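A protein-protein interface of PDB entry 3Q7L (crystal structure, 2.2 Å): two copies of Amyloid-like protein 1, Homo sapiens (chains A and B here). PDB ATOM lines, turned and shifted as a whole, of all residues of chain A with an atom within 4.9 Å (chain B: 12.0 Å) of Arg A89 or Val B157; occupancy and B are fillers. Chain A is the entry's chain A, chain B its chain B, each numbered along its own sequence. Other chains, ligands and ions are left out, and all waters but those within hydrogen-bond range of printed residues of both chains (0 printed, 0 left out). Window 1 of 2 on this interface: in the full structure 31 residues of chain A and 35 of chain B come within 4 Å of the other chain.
Arg A89 touches just these residues of chain B: Gln B152, Ala B156 and Val B157. Val B157 touches just one residue of chain A: Arg A89 (3.9 Å). No residue of chain B comes within 4 Å of Lys A34. No residue of chain B comes within 4 Å of Glu A88. No residue of chain B comes within 4 Å of Gln A90. No residue of chain B comes within 4 Å of Leu A92. No residue of chain B comes within 4 Å of Val A93. Printed residues of chain A within 4 Å of Ala B155: Ser A86. Of the printed residues of chain A, Pro B159 touches Ser A86 (2.9 Å). Tyr B151 touches none of the printed residues of chain A. Arg A91 touches none of the printed residues of chain B. The nearest printed residue of chain A that does not touch Val B157 is Ser A86 (5.5 Å).
The side-chain amide nitrogen of Gln B152 sits at hydrogen-bond distance from the backbone carbonyl oxygen of Arg B149 (3.1 Å).
Positions printed for both chains: 34, 89 and 93. Of the 8 pairs that touch across the chains among the printed residues, none has its exchanged pair printed and touching as well.
Among the printed residues, merely in contact across the chains: Val A85 with Gln B152 (3.8 Å), Val A85 with Ala B156 (3.7 Å), Ser A86 with Ala B155 (3.3 Å), Ser A86 with Ala B156 (3.96 Å), Ser A86 with Pro B159 (2.9 Å), Arg A89 with Gln B152 (3.8 Å), Arg A89 with Ala B156 (3.5 Å) and Arg A89 with Val B157 (3.9 Å).
Hydrophobic or aromatic side chains of chain A within 4 Å of the printed part of chain B: Val A85. Of the 21 printed residues of chain B, 5 touch a printed residue of chain A.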
ATOM      1  N   LYS A  34      -5.989 -12.697  25.134  1.00  0.00           N
ATOM      2  CA  LYS A  34      -7.141 -13.571  24.978  1.00  0.00           C
ATOM      3  C   LYS A  34      -7.858 -13.278  23.652  1.00  0.00           C
ATOM      4  O   LYS A  34      -8.280 -14.195  22.941  1.00  0.00           O
ATOM      5  CB  LYS A  34      -8.081 -13.347  26.153  1.00  0.00           C
ATOM      6  CG  LYS A  34      -9.256 -14.277  26.250  1.00  0.00           C
ATOM      7  CD  LYS A  34     -10.007 -13.909  27.513  1.00  0.00           C
ATOM      8  CE  LYS A  34     -11.407 -14.469  27.555  1.00  0.00           C
ATOM      9  NZ  LYS A  34     -12.055 -14.088  28.845  1.00  0.00           N
ATOM     10  N   VAL A  85      -7.030 -25.432  21.746  1.00  0.00           N
ATOM     11  CA  VAL A  85      -7.725 -24.223  22.176  1.00  0.00           C
ATOM     12  C   VAL A  85      -8.046 -24.320  23.668  1.00  0.00           C
ATOM     13  O   VAL A  85      -7.948 -23.336  24.396  1.00  0.00           O
ATOM     14  CB  VAL A  85      -9.039 -24.009  21.396  1.00  0.00           C
ATOM     15  CG1 VAL A  85      -9.856 -22.893  22.053  1.00  0.00           C
ATOM     16  CG2 VAL A  85      -8.729 -23.652  19.932  1.00  0.00           C
ATOM     17  N   SER A  86      -8.415 -25.512  24.126  1.00  0.00           N
ATOM     18  CA  SER A  86      -8.740 -25.710  25.530  1.00  0.00           C
ATOM     19  C   SER A  86      -7.503 -25.564  26.446  1.00  0.00           C
ATOM     20  O   SER A  86      -7.535 -24.825  27.422  1.00  0.00           O
ATOM     21  CB  SER A  86      -9.378 -27.092  25.712  1.00  0.00           C
ATOM     22  OG  SER A  86      -9.831 -27.282  27.037  1.00  0.00           O
ATOM     23  N   GLY A  87      -6.416 -26.260  26.120  1.00  0.00           N
ATOM     24  CA  GLY A  87      -5.215 -26.194  26.941  1.00  0.00           C
ATOM     25  C   GLY A  87      -4.614 -24.805  27.016  1.00  0.00           C
ATOM     26  O   GLY A  87      -4.083 -24.379  28.040  1.00  0.00           O
ATOM     27  N   GLU A  88      -4.710 -24.101  25.900  1.00  0.00           N
ATOM     28  CA  GLU A  88      -4.207 -22.750  25.758  1.00  0.00           C
ATOM     29  C   GLU A  88      -4.977 -21.792  26.671  1.00  0.00           C
ATOM     30  O   GLU A  88      -4.381 -20.963  27.358  1.00  0.00           O
ATOM     31  CB  GLU A  88      -4.355 -22.354  24.299  1.00  0.00           C
ATOM     32  CG  GLU A  88      -3.837 -21.019  23.894  1.00  0.00           C
ATOM     33  CD  GLU A  88      -3.996 -20.822  22.394  1.00  0.00           C
ATOM     34  OE1 GLU A  88      -5.150 -20.852  21.894  1.00  0.00           O
ATOM     35  OE2 GLU A  88      -2.969 -20.653  21.715  1.00  0.00           O
ATOM     36  N   ARG A  89      -6.303 -21.912  26.683  1.00  0.00           N
ATOM     37  CA  ARG A  89      -7.123 -21.042  27.519  1.00  0.00           C
ATOM     38  C   ARG A  89      -6.802 -21.295  28.988  1.00  0.00           C
ATOM     39  O   ARG A  89      -6.704 -20.362  29.781  1.00  0.00           O
ATOM     40  CB  ARG A  89      -8.616 -21.292  27.252  1.00  0.00           C
ATOM     41  CG  ARG A  89      -9.567 -20.599  28.232  1.00  0.00           C
ATOM     42  CD  ARG A  89      -9.376 -19.094  28.238  1.00  0.00           C
ATOM     43  NE  ARG A  89      -9.642 -18.465  26.941  1.00  0.00           N
ATOM     44  CZ  ARG A  89     -10.859 -18.209  26.470  1.00  0.00           C
ATOM     45  NH1 ARG A  89     -11.928 -18.525  27.184  1.00  0.00           N
ATOM     46  NH2 ARG A  89     -11.009 -17.622  25.294  1.00  0.00           N
ATOM     47  N   GLN A  90      -6.644 -22.568  29.339  1.00  0.00           N
ATOM     48  CA  GLN A  90      -6.324 -22.962  30.702  1.00  0.00           C
ATOM     49  C   GLN A  90      -5.020 -22.309  31.158  1.00  0.00           C
ATOM     50  O   GLN A  90      -4.919 -21.813  32.280  1.00  0.00           O
ATOM     51  CB  GLN A  90      -6.209 -24.486  30.793  1.00  0.00           C
ATOM     52  CG  GLN A  90      -7.359 -25.138  31.540  1.00  0.00           C
ATOM     53  CD  GLN A  90      -7.376 -26.650  31.390  1.00  0.00           C
ATOM     54  OE1 GLN A  90      -7.674 -27.177  30.314  1.00  0.00           O
ATOM     55  NE2 GLN A  90      -7.055 -27.356  32.470  1.00  0.00           N
ATOM     56  N   ARG A  91      -4.031 -22.311  30.270  1.00  0.00           N
ATOM     57  CA  ARG A  91      -2.728 -21.714  30.545  1.00  0.00           C
ATOM     58  C   ARG A  91      -2.859 -20.204  30.780  1.00  0.00           C
ATOM     59  O   ARG A  91      -2.286 -19.656  31.729  1.00  0.00           O
ATOM     60  CB  ARG A  91      -1.781 -22.000  29.369  1.00  0.00           C
ATOM     61  CG  ARG A  91      -0.393 -21.386  29.483  1.00  0.00           C
ATOM     62  CD  ARG A  91       0.639 -22.158  28.648  1.00  0.00           C
ATOM     63  NE  ARG A  91       1.990 -21.606  28.788  1.00  0.00           N
ATOM     64  CZ  ARG A  91       2.466 -20.586  28.076  1.00  0.00           C
ATOM     65  NH1 ARG A  91       1.706 -20.002  27.161  1.00  0.00           N
ATOM     66  NH2 ARG A  91       3.701 -20.143  28.284  1.00  0.00           N
ATOM     67  N   LEU A  92      -3.628 -19.539  29.924  1.00  0.00           N
ATOM     68  CA  LEU A  92      -3.841 -18.093  30.026  1.00  0.00           C
ATOM     69  C   LEU A  92      -4.546 -17.775  31.344  1.00  0.00           C
ATOM     70  O   LEU A  92      -4.111 -16.907  32.104  1.00  0.00           O
ATOM     71  CB  LEU A  92      -4.694 -17.604  28.847  1.00  0.00           C
ATOM     72  CG  LEU A  92      -4.848 -16.104  28.595  1.00  0.00           C
ATOM     73  CD1 LEU A  92      -3.545 -15.545  28.057  1.00  0.00           C
ATOM     74  CD2 LEU A  92      -5.963 -15.851  27.588  1.00  0.00           C
ATOM     75  N   VAL A  93      -5.637 -18.485  31.608  1.00  0.00           N
ATOM     76  CA  VAL A  93      -6.403 -18.295  32.834  1.00  0.00           C
ATOM     77  C   VAL A  93      -5.518 -18.456  34.087  1.00  0.00           C
ATOM     78  O   VAL A  93      -5.539 -17.611  34.975  1.00  0.00           O
ATOM     79  CB  VAL A  93      -7.584 -19.302  32.900  1.00  0.00           C
ATOM     80  CG1 VAL A  93      -8.145 -19.364  34.310  1.00  0.00           C
ATOM     81  CG2 VAL A  93      -8.689 -18.888  31.903  1.00  0.00           C
ATOM     82  N   GLU A  94      -4.745 -19.538  34.141  1.00  0.00           N
ATOM     83  CA  GLU A  94      -3.857 -19.823  35.268  1.00  0.00           C
ATOM     84  C   GLU A  94      -2.833 -18.705  35.469  1.00  0.00           C
ATOM     85  O   GLU A  94      -2.649 -18.212  36.580  1.00  0.00           O
ATOM     86  CB  GLU A  94      -3.128 -21.156  35.043  1.00  0.00           C
ATOM     87  CG  GLU A  94      -2.304 -21.637  36.229  1.00  0.00           C
ATOM     88  N   LYS B  34     -24.893  -7.454  34.421  1.00  0.00           N
ATOM     89  CA  LYS B  34     -24.019  -8.515  34.893  1.00  0.00           C
ATOM     90  C   LYS B  34     -23.214  -8.050  36.108  1.00  0.00           C
ATOM     91  O   LYS B  34     -23.087  -8.782  37.089  1.00  0.00           O
ATOM     92  CB  LYS B  34     -23.069  -8.929  33.774  1.00  0.00           C
ATOM     93  CG  LYS B  34     -22.298 -10.206  34.022  1.00  0.00           C
ATOM     94  CD  LYS B  34     -21.549 -10.590  32.753  1.00  0.00           C
ATOM     95  CE  LYS B  34     -20.811 -11.906  32.894  1.00  0.00           C
ATOM     96  NZ  LYS B  34     -20.122 -12.264  31.618  1.00  0.00           N
ATOM     97  N   ARG B  89     -27.336 -16.300  36.390  1.00  0.00           N
ATOM     98  CA  ARG B  89     -26.315 -16.094  35.371  1.00  0.00           C
ATOM     99  C   ARG B  89     -26.777 -16.695  34.048  1.00  0.00           C
ATOM    100  O   ARG B  89     -26.613 -16.102  32.986  1.00  0.00           O
ATOM    101  CB  ARG B  89     -25.000 -16.752  35.796  1.00  0.00           C
ATOM    102  CG  ARG B  89     -23.911 -16.715  34.722  1.00  0.00           C
ATOM    103  CD  ARG B  89     -23.660 -15.287  34.240  1.00  0.00           C
ATOM    104  NE  ARG B  89     -23.044 -14.436  35.255  1.00  0.00           N
ATOM    105  CZ  ARG B  89     -21.777 -14.535  35.645  1.00  0.00           C
ATOM    106  NH1 ARG B  89     -20.982 -15.452  35.107  1.00  0.00           N
ATOM    107  NH2 ARG B  89     -21.303 -13.709  36.569  1.00  0.00           N
ATOM    108  N   VAL B  93     -27.290 -14.863  30.555  1.00  0.00           N
ATOM    109  CA  VAL B  93     -26.562 -15.343  29.379  1.00  0.00           C
ATOM    110  C   VAL B  93     -27.474 -15.659  28.183  1.00  0.00           C
ATOM    111  O   VAL B  93     -27.197 -15.240  27.060  1.00  0.00           O
ATOM    112  CB  VAL B  93     -25.720 -16.600  29.733  1.00  0.00           C
ATOM    113  CG1 VAL B  93     -25.072 -17.174  28.485  1.00  0.00           C
ATOM    114  CG2 VAL B  93     -24.627 -16.232  30.736  1.00  0.00           C
ATOM    115  N   LEU B 148     -18.267 -18.911  14.231  1.00  0.00           N
ATOM    116  CA  LEU B 148     -16.911 -19.363  14.545  1.00  0.00           C
ATOM    117  C   LEU B 148     -16.551 -19.025  15.995  1.00  0.00           C
ATOM    118  O   LEU B 148     -16.083 -19.878  16.733  1.00  0.00           O
ATOM    119  CB  LEU B 148     -15.900 -18.716  13.594  1.00  0.00           C
ATOM    120  CG  LEU B 148     -15.959 -19.031  12.094  1.00  0.00           C
ATOM    121  CD1 LEU B 148     -15.082 -18.017  11.366  1.00  0.00           C
ATOM    122  CD2 LEU B 148     -15.477 -20.472  11.803  1.00  0.00           C
ATOM    123  N   ARG B 149     -16.786 -17.786  16.402  1.00  0.00           N
ATOM    124  CA  ARG B 149     -16.494 -17.366  17.766  1.00  0.00           C
ATOM    125  C   ARG B 149     -17.204 -18.206  18.838  1.00  0.00           C
ATOM    126  O   ARG B 149     -16.606 -18.542  19.860  1.00  0.00           O
ATOM    127  CB  ARG B 149     -16.866 -15.893  17.956  1.00  0.00           C
ATOM    128  CG  ARG B 149     -16.426 -15.319  19.309  1.00  0.00           C
ATOM    129  CD  ARG B 149     -16.768 -13.829  19.443  1.00  0.00           C
ATOM    130  NE  ARG B 149     -16.123 -13.013  18.416  1.00  0.00           N
ATOM    131  CZ  ARG B 149     -16.751 -12.485  17.361  1.00  0.00           C
ATOM    132  NH1 ARG B 149     -18.058 -12.680  17.176  1.00  0.00           N
ATOM    133  NH2 ARG B 149     -16.073 -11.755  16.487  1.00  0.00           N
ATOM    134  N   HIS B 150     -18.473 -18.545  18.618  1.00  0.00           N
ATOM    135  CA  HIS B 150     -19.218 -19.333  19.601  1.00  0.00           C
ATOM    136  C   HIS B 150     -18.589 -20.703  19.793  1.00  0.00           C
ATOM    137  O   HIS B 150     -18.453 -21.182  20.921  1.00  0.00           O
ATOM    138  CB  HIS B 150     -20.685 -19.500  19.184  1.00  0.00           C
ATOM    139  CG  HIS B 150     -21.471 -20.375  20.106  1.00  0.00           C
ATOM    140  ND1 HIS B 150     -22.262 -21.413  19.651  1.00  0.00           N
ATOM    141  CD2 HIS B 150     -21.578 -20.389  21.453  1.00  0.00           C
ATOM    142  CE1 HIS B 150     -22.816 -22.026  20.683  1.00  0.00           C
ATOM    143  NE2 HIS B 150     -22.416 -21.423  21.788  1.00  0.00           N
ATOM    144  N   TYR B 151     -18.223 -21.336  18.685  1.00  0.00           N
ATOM    145  CA  TYR B 151     -17.588 -22.649  18.708  1.00  0.00           C
ATOM    146  C   TYR B 151     -16.215 -22.563  19.380  1.00  0.00           C
ATOM    147  O   TYR B 151     -15.860 -23.403  20.205  1.00  0.00           O
ATOM    148  CB  TYR B 151     -17.441 -23.163  17.276  1.00  0.00           C
ATOM    149  CG  TYR B 151     -16.607 -24.412  17.115  1.00  0.00           C
ATOM    150  CD1 TYR B 151     -16.903 -25.575  17.829  1.00  0.00           C
ATOM    151  CD2 TYR B 151     -15.567 -24.453  16.183  1.00  0.00           C
ATOM    152  CE1 TYR B 151     -16.190 -26.754  17.615  1.00  0.00           C
ATOM    153  CE2 TYR B 151     -14.846 -25.618  15.957  1.00  0.00           C
ATOM    154  CZ  TYR B 151     -15.163 -26.768  16.668  1.00  0.00           C
ATOM    155  OH  TYR B 151     -14.481 -27.931  16.388  1.00  0.00           O
ATOM    156  N   GLN B 152     -15.446 -21.540  19.021  1.00  0.00           N
ATOM    157  CA  GLN B 152     -14.127 -21.342  19.596  1.00  0.00           C
ATOM    158  C   GLN B 152     -14.270 -21.165  21.109  1.00  0.00           C
ATOM    159  O   GLN B 152     -13.462 -21.674  21.884  1.00  0.00           O
ATOM    160  CB  GLN B 152     -13.462 -20.117  18.962  1.00  0.00           C
ATOM    161  CG  GLN B 152     -12.210 -19.653  19.677  1.00  0.00           C
ATOM    162  CD  GLN B 152     -12.498 -18.689  20.824  1.00  0.00           C
ATOM    163  OE1 GLN B 152     -11.634 -18.433  21.661  1.00  0.00           O
ATOM    164  NE2 GLN B 152     -13.709 -18.139  20.856  1.00  0.00           N
ATOM    165  N   HIS B 153     -15.316 -20.453  21.514  1.00  0.00           N
ATOM    166  CA  HIS B 153     -15.585 -20.220  22.925  1.00  0.00           C
ATOM    167  C   HIS B 153     -15.875 -21.520  23.667  1.00  0.00           C
ATOM    168  O   HIS B 153     -15.302 -21.776  24.723  1.00  0.00           O
ATOM    169  CB  HIS B 153     -16.774 -19.274  23.106  1.00  0.00           C
ATOM    170  CG  HIS B 153     -17.115 -19.020  24.538  1.00  0.00           C
ATOM    171  ND1 HIS B 153     -16.391 -18.146  25.329  1.00  0.00           N
ATOM    172  CD2 HIS B 153     -18.042 -19.578  25.352  1.00  0.00           C
ATOM    173  CE1 HIS B 153     -16.861 -18.187  26.565  1.00  0.00           C
ATOM    174  NE2 HIS B 153     -17.859 -19.047  26.605  1.00  0.00           N
ATOM    175  N   VAL B 154     -16.780 -22.330  23.136  1.00  0.00           N
ATOM    176  CA  VAL B 154     -17.109 -23.592  23.777  1.00  0.00           C
ATOM    177  C   VAL B 154     -15.878 -24.502  23.866  1.00  0.00           C
ATOM    178  O   VAL B 154     -15.707 -25.215  24.846  1.00  0.00           O
ATOM    179  CB  VAL B 154     -18.238 -24.339  23.025  1.00  0.00           C
ATOM    180  CG1 VAL B 154     -18.474 -25.689  23.655  1.00  0.00           C
ATOM    181  CG2 VAL B 154     -19.531 -23.531  23.080  1.00  0.00           C
ATOM    182  N   ALA B 155     -15.023 -24.484  22.845  1.00  0.00           N
ATOM    183  CA  ALA B 155     -13.822 -25.323  22.869  1.00  0.00           C
ATOM    184  C   ALA B 155     -12.840 -24.825  23.938  1.00  0.00           C
ATOM    185  O   ALA B 155     -12.091 -25.608  24.526  1.00  0.00           O
ATOM    186  CB  ALA B 155     -13.138 -25.326  21.504  1.00  0.00           C
ATOM    187  N   ALA B 156     -12.860 -23.521  24.184  1.00  0.00           N
ATOM    188  CA  ALA B 156     -11.973 -22.914  25.158  1.00  0.00           C
ATOM    189  C   ALA B 156     -12.323 -23.273  26.600  1.00  0.00           C
ATOM    190  O   ALA B 156     -11.429 -23.505  27.414  1.00  0.00           O
ATOM    191  CB  ALA B 156     -11.979 -21.395  24.984  1.00  0.00           C
ATOM    192  N   VAL B 157     -13.617 -23.321  26.915  1.00  0.00           N
ATOM    193  CA  VAL B 157     -14.043 -23.616  28.277  1.00  0.00           C
ATOM    194  C   VAL B 157     -14.709 -24.966  28.488  1.00  0.00           C
ATOM    195  O   VAL B 157     -14.849 -25.410  29.622  1.00  0.00           O
ATOM    196  CB  VAL B 157     -15.011 -22.531  28.808  1.00  0.00           C
ATOM    197  CG1 VAL B 157     -14.396 -21.147  28.627  1.00  0.00           C
ATOM    198  CG2 VAL B 157     -16.351 -22.632  28.095  1.00  0.00           C
ATOM    199  N   ASP B 158     -15.125 -25.623  27.411  1.00  0.00           N
ATOM    200  CA  ASP B 158     -15.800 -26.912  27.548  1.00  0.00           C
ATOM    201  C   ASP B 158     -15.567 -27.783  26.317  1.00  0.00           C
ATOM    202  O   ASP B 158     -16.399 -27.821  25.410  1.00  0.00           O
ATOM    203  CB  ASP B 158     -17.306 -26.689  27.748  1.00  0.00           C
ATOM    204  CG  ASP B 158     -18.048 -27.960  28.143  1.00  0.00           C
ATOM    205  OD1 ASP B 158     -17.604 -29.060  27.751  1.00  0.00           O
ATOM    206  OD2 ASP B 158     -19.087 -27.857  28.835  1.00  0.00           O
ATOM    207  N   PRO B 159     -14.431 -28.497  26.274  1.00  0.00           N
ATOM    208  CA  PRO B 159     -14.038 -29.384  25.173  1.00  0.00           C
ATOM    209  C   PRO B 159     -15.074 -30.448  24.784  1.00  0.00           C
ATOM    210  O   PRO B 159     -15.289 -30.709  23.599  1.00  0.00           O
ATOM    211  CB  PRO B 159     -12.745 -30.006  25.688  1.00  0.00           C
ATOM    212  CG  PRO B 159     -12.170 -28.918  26.528  1.00  0.00           C
ATOM    213  CD  PRO B 159     -13.370 -28.432  27.292  1.00  0.00           C
ATOM    214  N   GLU B 160     -15.708 -31.061  25.781  1.00  0.00           N
ATOM    215  CA  GLU B 160     -16.704 -32.104  25.533  1.00  0.00           C
ATOM    216  C   GLU B 160     -17.857 -31.588  24.688  1.00  0.00           C
ATOM    217  O   GLU B 160     -18.255 -32.223  23.707  1.00  0.00           O
ATOM    218  CB  GLU B 160     -17.236 -32.655  26.853  1.00  0.00           C
ATOM    219  N   LYS B 161     -18.395 -30.438  25.075  1.00  0.00           N
ATOM    220  CA  LYS B 161     -19.500 -29.833  24.347  1.00  0.00           C
ATOM    221  C   LYS B 161     -19.066 -29.384  22.947  1.00  0.00           C
ATOM    222  O   LYS B 161     -19.869 -29.381  22.015  1.00  0.00           O
ATOM    223  CB  LYS B 161     -20.067 -28.646  25.127  1.00  0.00           C
ATOM    224  N   ALA B 162     -17.793 -29.018  22.799  1.00  0.00           N
ATOM    225  CA  ALA B 162     -17.262 -28.567  21.513  1.00  0.00           C
ATOM    226  C   ALA B 162     -17.320 -29.674  20.467  1.00  0.00           C
ATOM    227  O   ALA B 162     -17.671 -29.428  19.311  1.00  0.00           O
ATOM    228  CB  ALA B 162     -15.816 -28.077  21.675  1.00  0.00           C
ATOM    229  N   GLN B 163     -16.972 -30.893  20.874  1.00  0.00           N
ATOM    230  CA  GLN B 163     -16.980 -32.040  19.971  1.00  0.00           C
ATOM    231  C   GLN B 163     -18.383 -32.351  19.455  1.00  0.00           C
ATOM    232  O   GLN B 163     -18.548 -32.837  18.335  1.00  0.00           O
ATOM    233  CB  GLN B 163     -16.434 -33.282  20.682  1.00  0.00           C
ATOM    234  CG  GLN B 163     -16.363 -34.514  19.786  1.00  0.00           C
ATOM    235  CD  GLN B 163     -16.079 -35.793  20.550  1.00  0.00           C
ATOM    236  OE1 GLN B 163     -16.934 -36.296  21.282  1.00  0.00           O
ATOM    237  NE2 GLN B 163     -14.872 -36.327  20.384  1.00  0.00           N
ATOM    238  N   GLN B 164     -19.383 -32.063  20.278  1.00  0.00           N
ATOM    239  CA  GLN B 164     -20.773 -32.331  19.939  1.00  0.00           C
ATOM    240  C   GLN B 164     -21.355 -31.364  18.906  1.00  0.00           C
ATOM    241  O   GLN B 164     -22.155 -31.768  18.057  1.00  0.00           O
ATOM    242  CB  GLN B 164     -21.635 -32.270  21.202  1.00  0.00           C
ATOM    243  CG  GLN B 164     -21.070 -33.017  22.399  1.00  0.00           C
ATOM    244  CD  GLN B 164     -21.854 -32.726  23.669  1.00  0.00           C
ATOM    245  OE1 GLN B 164     -22.019 -31.568  24.056  1.00  0.00           O
ATOM    246  NE2 GLN B 164     -22.343 -33.775  24.320  1.00  0.00           N
ATOM    247  N   MET B 165     -20.972 -30.092  18.985  1.00  0.00           N
ATOM    248  CA  MET B 165     -21.495 -29.095  18.053  1.00  0.00           C
ATOM    249  C   MET B 165     -20.693 -29.011  16.754  1.00  0.00           C
ATOM    250  O   MET B 165     -21.121 -28.386  15.787  1.00  0.00           O
ATOM    251  CB  MET B 165     -21.527 -27.723  18.734  1.00  0.00           C
ATOM    252  CG  MET B 165     -20.153 -27.164  19.058  1.00  0.00           C
ATOM    253  SD  MET B 165     -20.231 -25.735  20.166  1.00  0.00           S
ATOM    254  CE  MET B 165     -20.876 -24.439  19.067  1.00  0.00           C
